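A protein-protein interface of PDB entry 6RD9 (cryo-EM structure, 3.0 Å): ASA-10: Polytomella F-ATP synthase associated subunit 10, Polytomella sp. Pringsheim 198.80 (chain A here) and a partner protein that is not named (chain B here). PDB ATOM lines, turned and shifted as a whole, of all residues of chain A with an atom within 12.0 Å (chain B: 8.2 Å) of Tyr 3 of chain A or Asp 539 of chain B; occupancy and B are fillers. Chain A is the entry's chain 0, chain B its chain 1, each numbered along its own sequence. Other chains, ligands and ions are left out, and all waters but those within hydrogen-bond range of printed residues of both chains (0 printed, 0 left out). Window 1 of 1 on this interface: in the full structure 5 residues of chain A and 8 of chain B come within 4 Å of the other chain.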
ATOM      1  N   SER A   2      33.164 -13.682  -2.246  1.00  0.00           N
ATOM      2  CA  SER A   2      31.954 -14.436  -2.460  1.00  0.00           C
ATOM      3  C   SER A   2      30.885 -13.462  -2.825  1.00  0.00           C
ATOM      4  O   SER A   2      30.251 -12.903  -1.953  1.00  0.00           O
ATOM      5  CB  SER A   2      31.585 -15.236  -1.219  1.00  0.00           C
ATOM      6  OG  SER A   2      32.413 -16.377  -1.088  1.00  0.00           O
ATOM      7  N   TYR A   3      30.781 -13.190  -4.125  1.00  0.00           N
ATOM      8  CA  TYR A   3      29.788 -12.349  -4.796  1.00  0.00           C
ATOM      9  C   TYR A   3      29.887 -10.873  -4.458  1.00  0.00           C
ATOM     10  O   TYR A   3      29.178 -10.081  -5.061  1.00  0.00           O
ATOM     11  CB  TYR A   3      28.358 -12.802  -4.513  1.00  0.00           C
ATOM     12  CG  TYR A   3      27.952 -14.063  -5.190  1.00  0.00           C
ATOM     13  CD1 TYR A   3      28.341 -14.325  -6.468  1.00  0.00           C
ATOM     14  CD2 TYR A   3      27.177 -14.992  -4.538  1.00  0.00           C
ATOM     15  CE1 TYR A   3      27.990 -15.478  -7.066  1.00  0.00           C
ATOM     16  CE2 TYR A   3      26.819 -16.136  -5.139  1.00  0.00           C
ATOM     17  CZ  TYR A   3      27.234 -16.373  -6.401  1.00  0.00           C
ATOM     18  OH  TYR A   3      26.900 -17.526  -7.038  1.00  0.00           O
ATOM     19  N   SER A   4      30.747 -10.470  -3.527  1.00  0.00           N
ATOM     20  CA  SER A   4      30.897  -9.049  -3.251  1.00  0.00           C
ATOM     21  C   SER A   4      31.634  -8.350  -4.367  1.00  0.00           C
ATOM     22  O   SER A   4      31.364  -7.188  -4.651  1.00  0.00           O
ATOM     23  CB  SER A   4      31.643  -8.823  -1.947  1.00  0.00           C
ATOM     24  OG  SER A   4      30.853  -9.155  -0.835  1.00  0.00           O
ATOM     25  N   ALA A   5      32.556  -9.037  -5.007  1.00  0.00           N
ATOM     26  CA  ALA A   5      33.327  -8.481  -6.096  1.00  0.00           C
ATOM     27  C   ALA A   5      32.620  -8.563  -7.430  1.00  0.00           C
ATOM     28  O   ALA A   5      33.139  -8.047  -8.415  1.00  0.00           O
ATOM     29  CB  ALA A   5      34.653  -9.207  -6.186  1.00  0.00           C
ATOM     30  N   TYR A   6      31.484  -9.235  -7.500  1.00  0.00           N
ATOM     31  CA  TYR A   6      30.691  -9.223  -8.714  1.00  0.00           C
ATOM     32  C   TYR A   6      29.835  -7.977  -8.789  1.00  0.00           C
ATOM     33  O   TYR A   6      29.551  -7.479  -9.879  1.00  0.00           O
ATOM     34  CB  TYR A   6      29.827 -10.474  -8.766  1.00  0.00           C
ATOM     35  CG  TYR A   6      28.776 -10.461  -9.817  1.00  0.00           C
ATOM     36  CD1 TYR A   6      29.110 -10.474 -11.142  1.00  0.00           C
ATOM     37  CD2 TYR A   6      27.452 -10.428  -9.483  1.00  0.00           C
ATOM     38  CE1 TYR A   6      28.149 -10.453 -12.103  1.00  0.00           C
ATOM     39  CE2 TYR A   6      26.491 -10.412 -10.431  1.00  0.00           C
ATOM     40  CZ  TYR A   6      26.840 -10.422 -11.739  1.00  0.00           C
ATOM     41  OH  TYR A   6      25.874 -10.401 -12.703  1.00  0.00           O
ATOM     42  N   PHE A   7      29.432  -7.460  -7.643  1.00  0.00           N
ATOM     43  CA  PHE A   7      28.603  -6.278  -7.572  1.00  0.00           C
ATOM     44  C   PHE A   7      29.398  -4.997  -7.543  1.00  0.00           C
ATOM     45  O   PHE A   7      28.814  -3.926  -7.699  1.00  0.00           O
ATOM     46  CB  PHE A   7      27.710  -6.357  -6.353  1.00  0.00           C
ATOM     47  CG  PHE A   7      26.690  -7.403  -6.462  1.00  0.00           C
ATOM     48  CD1 PHE A   7      25.849  -7.433  -7.547  1.00  0.00           C
ATOM     49  CD2 PHE A   7      26.584  -8.368  -5.513  1.00  0.00           C
ATOM     50  CE1 PHE A   7      24.929  -8.401  -7.661  1.00  0.00           C
ATOM     51  CE2 PHE A   7      25.664  -9.335  -5.633  1.00  0.00           C
ATOM     52  CZ  PHE A   7      24.841  -9.348  -6.704  1.00  0.00           C
ATOM     53  N   ALA A   8      30.703  -5.075  -7.350  1.00  0.00           N
ATOM     54  CA  ALA A   8      31.528  -3.896  -7.503  1.00  0.00           C
ATOM     55  C   ALA A   8      31.919  -3.648  -8.946  1.00  0.00           C
ATOM     56  O   ALA A   8      32.397  -2.559  -9.257  1.00  0.00           O
ATOM     57  CB  ALA A   8      32.773  -4.027  -6.638  1.00  0.00           C
ATOM     58  N   LYS A   9      31.721  -4.622  -9.829  1.00  0.00           N
ATOM     59  CA  LYS A   9      32.153  -4.494 -11.214  1.00  0.00           C
ATOM     60  C   LYS A   9      31.262  -3.550 -11.995  1.00  0.00           C
ATOM     61  O   LYS A   9      31.748  -2.634 -12.661  1.00  0.00           O
ATOM     62  CB  LYS A   9      32.178  -5.857 -11.889  1.00  0.00           C
ATOM     63  CG  LYS A   9      33.305  -6.713 -11.422  1.00  0.00           C
ATOM     64  CD  LYS A   9      33.210  -8.084 -12.019  1.00  0.00           C
ATOM     65  CE  LYS A   9      34.266  -8.976 -11.438  1.00  0.00           C
ATOM     66  NZ  LYS A   9      34.433 -10.178 -12.272  1.00  0.00           N
ATOM     67  N   ALA A  10      29.962  -3.784 -11.974  1.00  0.00           N
ATOM     68  CA  ALA A  10      29.039  -2.825 -12.557  1.00  0.00           C
ATOM     69  C   ALA A  10      28.923  -1.644 -11.613  1.00  0.00           C
ATOM     70  O   ALA A  10      28.562  -1.810 -10.447  1.00  0.00           O
ATOM     71  CB  ALA A  10      27.681  -3.463 -12.805  1.00  0.00           C
ATOM     72  N   GLY A  11      29.271  -0.463 -12.092  1.00  0.00           N
ATOM     73  CA  GLY A  11      29.350   0.671 -11.206  1.00  0.00           C
ATOM     74  C   GLY A  11      28.018   1.346 -11.005  1.00  0.00           C
ATOM     75  O   GLY A  11      27.023   0.687 -10.711  1.00  0.00           O
ATOM     76  N   LYS B 309      31.465 -19.622   7.971  1.00  0.00           N
ATOM     77  CA  LYS B 309      31.300 -18.266   8.463  1.00  0.00           C
ATOM     78  C   LYS B 309      29.905 -18.113   9.027  1.00  0.00           C
ATOM     79  O   LYS B 309      28.946 -18.633   8.462  1.00  0.00           O
ATOM     80  CB  LYS B 309      31.520 -17.248   7.356  1.00  0.00           C
ATOM     81  CG  LYS B 309      32.917 -17.222   6.834  1.00  0.00           C
ATOM     82  CD  LYS B 309      33.198 -15.944   6.099  1.00  0.00           C
ATOM     83  CE  LYS B 309      32.353 -15.833   4.850  1.00  0.00           C
ATOM     84  NZ  LYS B 309      32.641 -14.590   4.077  1.00  0.00           N
ATOM     85  N   GLN B 313      29.133 -12.787  10.125  1.00  0.00           N
ATOM     86  CA  GLN B 313      30.437 -12.782   9.497  1.00  0.00           C
ATOM     87  C   GLN B 313      30.318 -12.838   7.990  1.00  0.00           C
ATOM     88  O   GLN B 313      31.237 -12.433   7.281  1.00  0.00           O
ATOM     89  CB  GLN B 313      31.214 -13.957  10.061  1.00  0.00           C
ATOM     90  CG  GLN B 313      32.631 -14.131   9.719  1.00  0.00           C
ATOM     91  CD  GLN B 313      33.247 -15.152  10.632  1.00  0.00           C
ATOM     92  OE1 GLN B 313      32.635 -15.562  11.608  1.00  0.00           O
ATOM     93  NE2 GLN B 313      34.445 -15.600  10.305  1.00  0.00           N
ATOM     94  N   ARG B 314      29.214 -13.368   7.482  1.00  0.00           N
ATOM     95  CA  ARG B 314      28.929 -13.290   6.058  1.00  0.00           C
ATOM     96  C   ARG B 314      28.311 -11.963   5.686  1.00  0.00           C
ATOM     97  O   ARG B 314      28.406 -11.556   4.530  1.00  0.00           O
ATOM     98  CB  ARG B 314      27.993 -14.411   5.629  1.00  0.00           C
ATOM     99  CG  ARG B 314      28.603 -15.755   5.626  1.00  0.00           C
ATOM    100  CD  ARG B 314      27.732 -16.733   4.921  1.00  0.00           C
ATOM    101  NE  ARG B 314      26.358 -16.659   5.371  1.00  0.00           N
ATOM    102  CZ  ARG B 314      25.806 -17.501   6.226  1.00  0.00           C
ATOM    103  NH1 ARG B 314      26.510 -18.491   6.726  1.00  0.00           N
ATOM    104  NH2 ARG B 314      24.545 -17.368   6.570  1.00  0.00           N
ATOM    105  N   LEU B 315      27.664 -11.292   6.632  1.00  0.00           N
ATOM    106  CA  LEU B 315      27.177  -9.944   6.402  1.00  0.00           C
ATOM    107  C   LEU B 315      28.278  -8.910   6.421  1.00  0.00           C
ATOM    108  O   LEU B 315      28.115  -7.855   5.834  1.00  0.00           O
ATOM    109  CB  LEU B 315      26.155  -9.552   7.453  1.00  0.00           C
ATOM    110  CG  LEU B 315      24.682  -9.712   7.150  1.00  0.00           C
ATOM    111  CD1 LEU B 315      23.936  -9.143   8.291  1.00  0.00           C
ATOM    112  CD2 LEU B 315      24.328  -8.984   5.908  1.00  0.00           C
ATOM    113  N   ASN B 316      29.378  -9.161   7.111  1.00  0.00           N
ATOM    114  CA  ASN B 316      30.443  -8.175   7.172  1.00  0.00           C
ATOM    115  C   ASN B 316      31.194  -8.081   5.868  1.00  0.00           C
ATOM    116  O   ASN B 316      31.749  -7.030   5.547  1.00  0.00           O
ATOM    117  CB  ASN B 316      31.404  -8.533   8.276  1.00  0.00           C
ATOM    118  CG  ASN B 316      30.946  -8.057   9.580  1.00  0.00           C
ATOM    119  OD1 ASN B 316      31.000  -8.766  10.570  1.00  0.00           O
ATOM    120  ND2 ASN B 316      30.493  -6.835   9.609  1.00  0.00           N
ATOM    121  N   SER B 317      31.254  -9.171   5.125  1.00  0.00           N
ATOM    122  CA  SER B 317      31.868  -9.184   3.816  1.00  0.00           C
ATOM    123  C   SER B 317      30.856  -8.991   2.707  1.00  0.00           C
ATOM    124  O   SER B 317      31.184  -9.207   1.537  1.00  0.00           O
ATOM    125  CB  SER B 317      32.631 -10.482   3.624  1.00  0.00           C
ATOM    126  OG  SER B 317      31.740 -11.571   3.654  1.00  0.00           O
ATOM    127  N   SER B 318      29.632  -8.605   3.052  1.00  0.00           N
ATOM    128  CA  SER B 318      28.609  -8.252   2.092  1.00  0.00           C
ATOM    129  C   SER B 318      28.994  -6.960   1.393  1.00  0.00           C
ATOM    130  O   SER B 318      29.816  -6.200   1.902  1.00  0.00           O
ATOM    131  CB  SER B 318      27.280  -8.072   2.809  1.00  0.00           C
ATOM    132  OG  SER B 318      26.182  -8.047   1.937  1.00  0.00           O
ATOM    133  N   PRO B 319      28.413  -6.677   0.226  1.00  0.00           N
ATOM    134  CA  PRO B 319      28.611  -5.356  -0.375  1.00  0.00           C
ATOM    135  C   PRO B 319      28.006  -4.222   0.416  1.00  0.00           C
ATOM    136  O   PRO B 319      28.333  -3.069   0.150  1.00  0.00           O
ATOM    137  CB  PRO B 319      27.941  -5.499  -1.737  1.00  0.00           C
ATOM    138  CG  PRO B 319      28.012  -6.894  -2.030  1.00  0.00           C
ATOM    139  CD  PRO B 319      27.883  -7.624  -0.762  1.00  0.00           C
ATOM    140  N   ALA B 320      27.133  -4.502   1.372  1.00  0.00           N
ATOM    141  CA  ALA B 320      26.509  -3.442   2.139  1.00  0.00           C
ATOM    142  C   ALA B 320      27.455  -2.825   3.133  1.00  0.00           C
ATOM    143  O   ALA B 320      27.299  -1.659   3.480  1.00  0.00           O
ATOM    144  CB  ALA B 320      25.308  -3.980   2.882  1.00  0.00           C
ATOM    145  N   HIS B 531      23.151 -23.400  -1.370  1.00  0.00           N
ATOM    146  CA  HIS B 531      23.779 -22.214  -1.907  1.00  0.00           C
ATOM    147  C   HIS B 531      22.862 -21.018  -1.871  1.00  0.00           C
ATOM    148  O   HIS B 531      23.336 -19.900  -1.708  1.00  0.00           O
ATOM    149  CB  HIS B 531      24.229 -22.461  -3.327  1.00  0.00           C
ATOM    150  CG  HIS B 531      25.068 -21.364  -3.877  1.00  0.00           C
ATOM    151  ND1 HIS B 531      24.648 -20.557  -4.900  1.00  0.00           N
ATOM    152  CD2 HIS B 531      26.287 -20.917  -3.521  1.00  0.00           C
ATOM    153  CE1 HIS B 531      25.584 -19.675  -5.172  1.00  0.00           C
ATOM    154  NE2 HIS B 531      26.592 -19.873  -4.351  1.00  0.00           N
ATOM    155  N   ILE B 532      21.561 -21.221  -2.028  1.00  0.00           N
ATOM    156  CA  ILE B 532      20.621 -20.135  -1.818  1.00  0.00           C
ATOM    157  C   ILE B 532      20.640 -19.708  -0.367  1.00  0.00           C
ATOM    158  O   ILE B 532      20.837 -18.536  -0.073  1.00  0.00           O
ATOM    159  CB  ILE B 532      19.215 -20.540  -2.267  1.00  0.00           C
ATOM    160  CG1 ILE B 532      19.210 -20.813  -3.747  1.00  0.00           C
ATOM    161  CG2 ILE B 532      18.294 -19.445  -2.050  1.00  0.00           C
ATOM    162  CD1 ILE B 532      17.930 -21.349  -4.253  1.00  0.00           C
ATOM    163  N   LYS B 534      22.833 -20.009   1.984  1.00  0.00           N
ATOM    164  CA  LYS B 534      24.077 -19.405   2.423  1.00  0.00           C
ATOM    165  C   LYS B 534      24.179 -17.960   1.983  1.00  0.00           C
ATOM    166  O   LYS B 534      24.827 -17.156   2.648  1.00  0.00           O
ATOM    167  CB  LYS B 534      25.223 -20.222   1.856  1.00  0.00           C
ATOM    168  CG  LYS B 534      26.581 -19.899   2.337  1.00  0.00           C
ATOM    169  CD  LYS B 534      27.584 -20.607   1.500  1.00  0.00           C
ATOM    170  CE  LYS B 534      28.948 -20.072   1.773  1.00  0.00           C
ATOM    171  NZ  LYS B 534      29.948 -20.670   0.843  1.00  0.00           N
ATOM    172  N   HIS B 535      23.529 -17.608   0.884  1.00  0.00           N
ATOM    173  CA  HIS B 535      23.739 -16.343   0.215  1.00  0.00           C
ATOM    174  C   HIS B 535      22.496 -15.492   0.057  1.00  0.00           C
ATOM    175  O   HIS B 535      22.634 -14.349  -0.357  1.00  0.00           O
ATOM    176  CB  HIS B 535      24.322 -16.579  -1.180  1.00  0.00           C
ATOM    177  CG  HIS B 535      25.761 -16.971  -1.181  1.00  0.00           C
ATOM    178  ND1 HIS B 535      26.765 -16.098  -0.845  1.00  0.00           N
ATOM    179  CD2 HIS B 535      26.367 -18.131  -1.501  1.00  0.00           C
ATOM    180  CE1 HIS B 535      27.926 -16.710  -0.933  1.00  0.00           C
ATOM    181  NE2 HIS B 535      27.712 -17.945  -1.332  1.00  0.00           N
ATOM    182  N   PHE B 536      21.303 -16.002   0.330  1.00  0.00           N
ATOM    183  CA  PHE B 536      20.092 -15.226   0.110  1.00  0.00           C
ATOM    184  C   PHE B 536      19.982 -14.130   1.139  1.00  0.00           C
ATOM    185  O   PHE B 536      20.123 -14.379   2.335  1.00  0.00           O
ATOM    186  CB  PHE B 536      18.863 -16.110   0.199  1.00  0.00           C
ATOM    187  CG  PHE B 536      17.625 -15.455  -0.245  1.00  0.00           C
ATOM    188  CD1 PHE B 536      17.377 -15.267  -1.570  1.00  0.00           C
ATOM    189  CD2 PHE B 536      16.701 -15.031   0.664  1.00  0.00           C
ATOM    190  CE1 PHE B 536      16.253 -14.664  -1.967  1.00  0.00           C
ATOM    191  CE2 PHE B 536      15.590 -14.433   0.261  1.00  0.00           C
ATOM    192  CZ  PHE B 536      15.361 -14.249  -1.053  1.00  0.00           C
ATOM    193  N   GLY B 537      19.709 -12.917   0.681  1.00  0.00           N
ATOM    194  CA  GLY B 537      19.601 -11.797   1.570  1.00  0.00           C
ATOM    195  C   GLY B 537      20.919 -11.246   2.025  1.00  0.00           C
ATOM    196  O   GLY B 537      20.941 -10.369   2.887  1.00  0.00           O
ATOM    197  N   ILE B 538      22.022 -11.744   1.491  1.00  0.00           N
ATOM    198  CA  ILE B 538      23.338 -11.221   1.802  1.00  0.00           C
ATOM    199  C   ILE B 538      23.980 -10.767   0.509  1.00  0.00           C
ATOM    200  O   ILE B 538      24.158  -9.571   0.295  1.00  0.00           O
ATOM    201  CB  ILE B 538      24.203 -12.263   2.523  1.00  0.00           C
ATOM    202  CG1 ILE B 538      23.633 -12.572   3.888  1.00  0.00           C
ATOM    203  CG2 ILE B 538      25.562 -11.755   2.721  1.00  0.00           C
ATOM    204  CD1 ILE B 538      24.055 -13.865   4.407  1.00  0.00           C
ATOM    205  N   ASP B 539      24.305 -11.689  -0.381  1.00  0.00           N
ATOM    206  CA  ASP B 539      24.941 -11.261  -1.615  1.00  0.00           C
ATOM    207  C   ASP B 539      24.540 -12.047  -2.847  1.00  0.00           C
ATOM    208  O   ASP B 539      25.245 -11.955  -3.845  1.00  0.00           O
ATOM    209  CB  ASP B 539      26.468 -11.285  -1.503  1.00  0.00           C
ATOM    210  CG  ASP B 539      27.010 -12.541  -0.845  1.00  0.00           C
ATOM    211  OD1 ASP B 539      26.434 -13.620  -1.002  1.00  0.00           O
ATOM    212  OD2 ASP B 539      28.043 -12.456  -0.163  1.00  0.00           O
ATOM    213  N   LEU B 540      23.481 -12.820  -2.824  1.00  0.00           N
ATOM    214  CA  LEU B 540      23.170 -13.653  -3.974  1.00  0.00           C
ATOM    215  C   LEU B 540      22.600 -12.785  -5.074  1.00  0.00           C
ATOM    216  O   LEU B 540      21.699 -12.004  -4.812  1.00  0.00           O
ATOM    217  CB  LEU B 540      22.164 -14.719  -3.591  1.00  0.00           C
ATOM    218  CG  LEU B 540      21.725 -15.884  -4.465  1.00  0.00           C
ATOM    219  CD1 LEU B 540      22.839 -16.746  -4.818  1.00  0.00           C
ATOM    220  CD2 LEU B 540      20.767 -16.641  -3.690  1.00  0.00           C
ATOM    221  N   PRO B 541      23.108 -12.854  -6.290  1.00  0.00           N
ATOM    222  CA  PRO B 541      22.481 -12.103  -7.358  1.00  0.00           C
ATOM    223  C   PRO B 541      21.188 -12.747  -7.793  1.00  0.00           C
ATOM    224  O   PRO B 541      20.928 -13.917  -7.556  1.00  0.00           O
ATOM    225  CB  PRO B 541      23.525 -12.132  -8.469  1.00  0.00           C
ATOM    226  CG  PRO B 541      24.423 -13.101  -8.132  1.00  0.00           C
ATOM    227  CD  PRO B 541      24.435 -13.299  -6.697  1.00  0.00           C
ATOM    228  N   HIS B 542      20.351 -11.950  -8.418  1.00  0.00           N
ATOM    229  CA  HIS B 542      19.128 -12.466  -8.983  1.00  0.00           C
ATOM    230  C   HIS B 542      19.356 -13.295 -10.219  1.00  0.00           C
ATOM    231  O   HIS B 542      18.444 -13.999 -10.644  1.00  0.00           O
ATOM    232  CB  HIS B 542      18.211 -11.320  -9.328  1.00  0.00           C
ATOM    233  CG  HIS B 542      17.315 -10.904  -8.219  1.00  0.00           C
ATOM    234  ND1 HIS B 542      17.768 -10.213  -7.128  1.00  0.00           N
ATOM    235  CD2 HIS B 542      15.983 -11.005  -8.072  1.00  0.00           C
ATOM    236  CE1 HIS B 542      16.759  -9.945  -6.330  1.00  0.00           C
ATOM    237  NE2 HIS B 542      15.663 -10.411  -6.883  1.00  0.00           N
ATOM    238  N   SER B 543      20.529 -13.205 -10.827  1.00  0.00           N
ATOM    239  CA  SER B 543      20.813 -14.007 -12.002  1.00  0.00           C
ATOM    240  C   SER B 543      21.122 -15.430 -11.631  1.00  0.00           C
ATOM    241  O   SER B 543      20.910 -16.335 -12.432  1.00  0.00           O
ATOM    242  CB  SER B 543      21.985 -13.423 -12.745  1.00  0.00           C
ATOM    243  OG  SER B 543      22.956 -12.999 -11.830  1.00  0.00           O
ATOM    244  N   VAL B 544      21.655 -15.636 -10.434  1.00  0.00           N
ATOM    245  CA  VAL B 544      22.040 -16.954  -9.974  1.00  0.00           C
ATOM    246  C   VAL B 544      20.835 -17.699  -9.462  1.00  0.00           C
ATOM    247  O   VAL B 544      20.732 -18.908  -9.641  1.00  0.00           O
ATOM    248  CB  VAL B 544      23.153 -16.806  -8.931  1.00  0.00           C
ATOM    249  CG1 VAL B 544      23.447 -18.064  -8.251  1.00  0.00           C
ATOM    250  CG2 VAL B 544      24.370 -16.410  -9.624  1.00  0.00           C
ATOM    251  N   VAL B 545      19.881 -16.992  -8.873  1.00  0.00           N
ATOM    252  CA  VAL B 545      18.613 -17.593  -8.484  1.00  0.00           C
ATOM    253  C   VAL B 545      17.855 -18.066  -9.708  1.00  0.00           C
ATOM    254  O   VAL B 545      17.354 -19.187  -9.755  1.00  0.00           O
ATOM    255  CB  VAL B 545      17.782 -16.583  -7.691  1.00  0.00           C
ATOM    256  CG1 VAL B 545      16.448 -17.113  -7.463  1.00  0.00           C
ATOM    257  CG2 VAL B 545      18.418 -16.287  -6.428  1.00  0.00           C
ATOM    258  N   MET B 548      19.722 -21.156 -11.111  1.00  0.00           N
ATOM    259  CA  MET B 548      19.534 -22.352 -10.317  1.00  0.00           C
ATOM    260  C   MET B 548      18.095 -22.813 -10.339  1.00  0.00           C
ATOM    261  O   MET B 548      17.822 -23.997 -10.517  1.00  0.00           O
ATOM    262  CB  MET B 548      19.960 -22.083  -8.891  1.00  0.00           C
ATOM    263  CG  MET B 548      21.370 -22.254  -8.625  1.00  0.00           C
ATOM    264  SD  MET B 548      21.515 -22.410  -6.880  1.00  0.00           S
ATOM    265  CE  MET B 548      21.598 -20.719  -6.468  1.00  0.00           C
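Of the 24 printed residues of chain B, 8 touch a printed residue of chain A.
The side-chain amino group of Lys 309 of chain B sits at hydrogen-bond distance from the side-chain hydroxyl of Ser 317 of chain B. The backbone carbonyl oxygen of Arg 314 of chain B lies within hydrogen-bond range of the side-chain hydroxyl of Ser 317 of chain B, 3.4 Å away. The backbone carbonyl oxygen (O) of Ile 538 of chain B is in hydrogen-bond range of the side-chain hydroxyl (OG) of Ser 318 of chain B, 3.0 Å away. The side-chain carboxylate of Asp 539 of chain B lies within hydrogen-bond range of a ring nitrogen (ND1) of His 535 of chain B, at 2.5 Å. N of Leu 540 of chain B lies within hydrogen-bond range of O of His 535 of chain B (3.0 Å).
Printed residues of chain B within 4 Å of Ser 2 of chain A: His 535 (3.96 Å) and Asp 539 (2.9 Å). Of chain B, only His 531 (3.1 Å), His 535 (3.9 Å), Asp 539 (3.3 Å), Pro 541 (3.9 Å) and Val 544 (3.7 Å) come within 4 Å of Tyr 3 of chain A. Of chain B, only Ser 317 (2.4 Å), Ser 318 (3.6 Å) and Pro 319 (3.3 Å) come within 4 Å of Ser 4 of chain A. Of the printed residues of chain B, Tyr 6 of chain A touches Pro 541. Leu 315 of chain B touches none of the printed residues of chain A. Of chain A, only Ser 2 and Tyr 3 come within 4 Å of His 535 of chain B. No residue of chain A comes within 4 Å of Gly 537 of chain B. No residue of chain A comes within 4 Å of Ile 538 of chain B. Of chain A, only Ser 2 (2.9 Å), Tyr 3 (3.3 Å) and Phe 7 (3.2 Å) come within 4 Å of Asp 539 of chain B. No residue of chain A comes within 4 Å of Leu 540 of chain B. Pro 541 of chain B touches just these residues of chain A: Tyr 3 (3.9 Å), Tyr 6 (3.95 Å) and Phe 7 (3.5 Å). Of chain A, only Tyr 3 comes within 4 Å of Val 544 of chain B. The nearest residue of chain A that does not touch Asp 539 of chain B is Ser 4 of chain A (4.4 Å).
O of Ser 2 of chain A lies close to OD2 of Asp 539 of chain B (2.9 Å). OG of Ser 4 of chain A lies close to O of Ser 317 of chain B.
Among the printed residues, pairs that only touch across the chains: Tyr 3 of chain A with His 531 of chain B, Phe 7 of chain A with Asp 539 of chain B, Tyr 3 of chain A with Asp 539 of chain B, Ser 4 of chain A with Pro 319 of chain B, Phe 7 of chain A with Pro 541 of chain B, Ser 4 of chain A with Ser 318 of chain B, Tyr 3 of chain A with Val 544 of chain B, Tyr 3 of chain A with His 535 of chain B, Tyr 3 of chain A with Pro 541 of chain B, Tyr 6 of chain A with Pro 541 of chain B and Ser 2 of chain A with His 535 of chain B.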
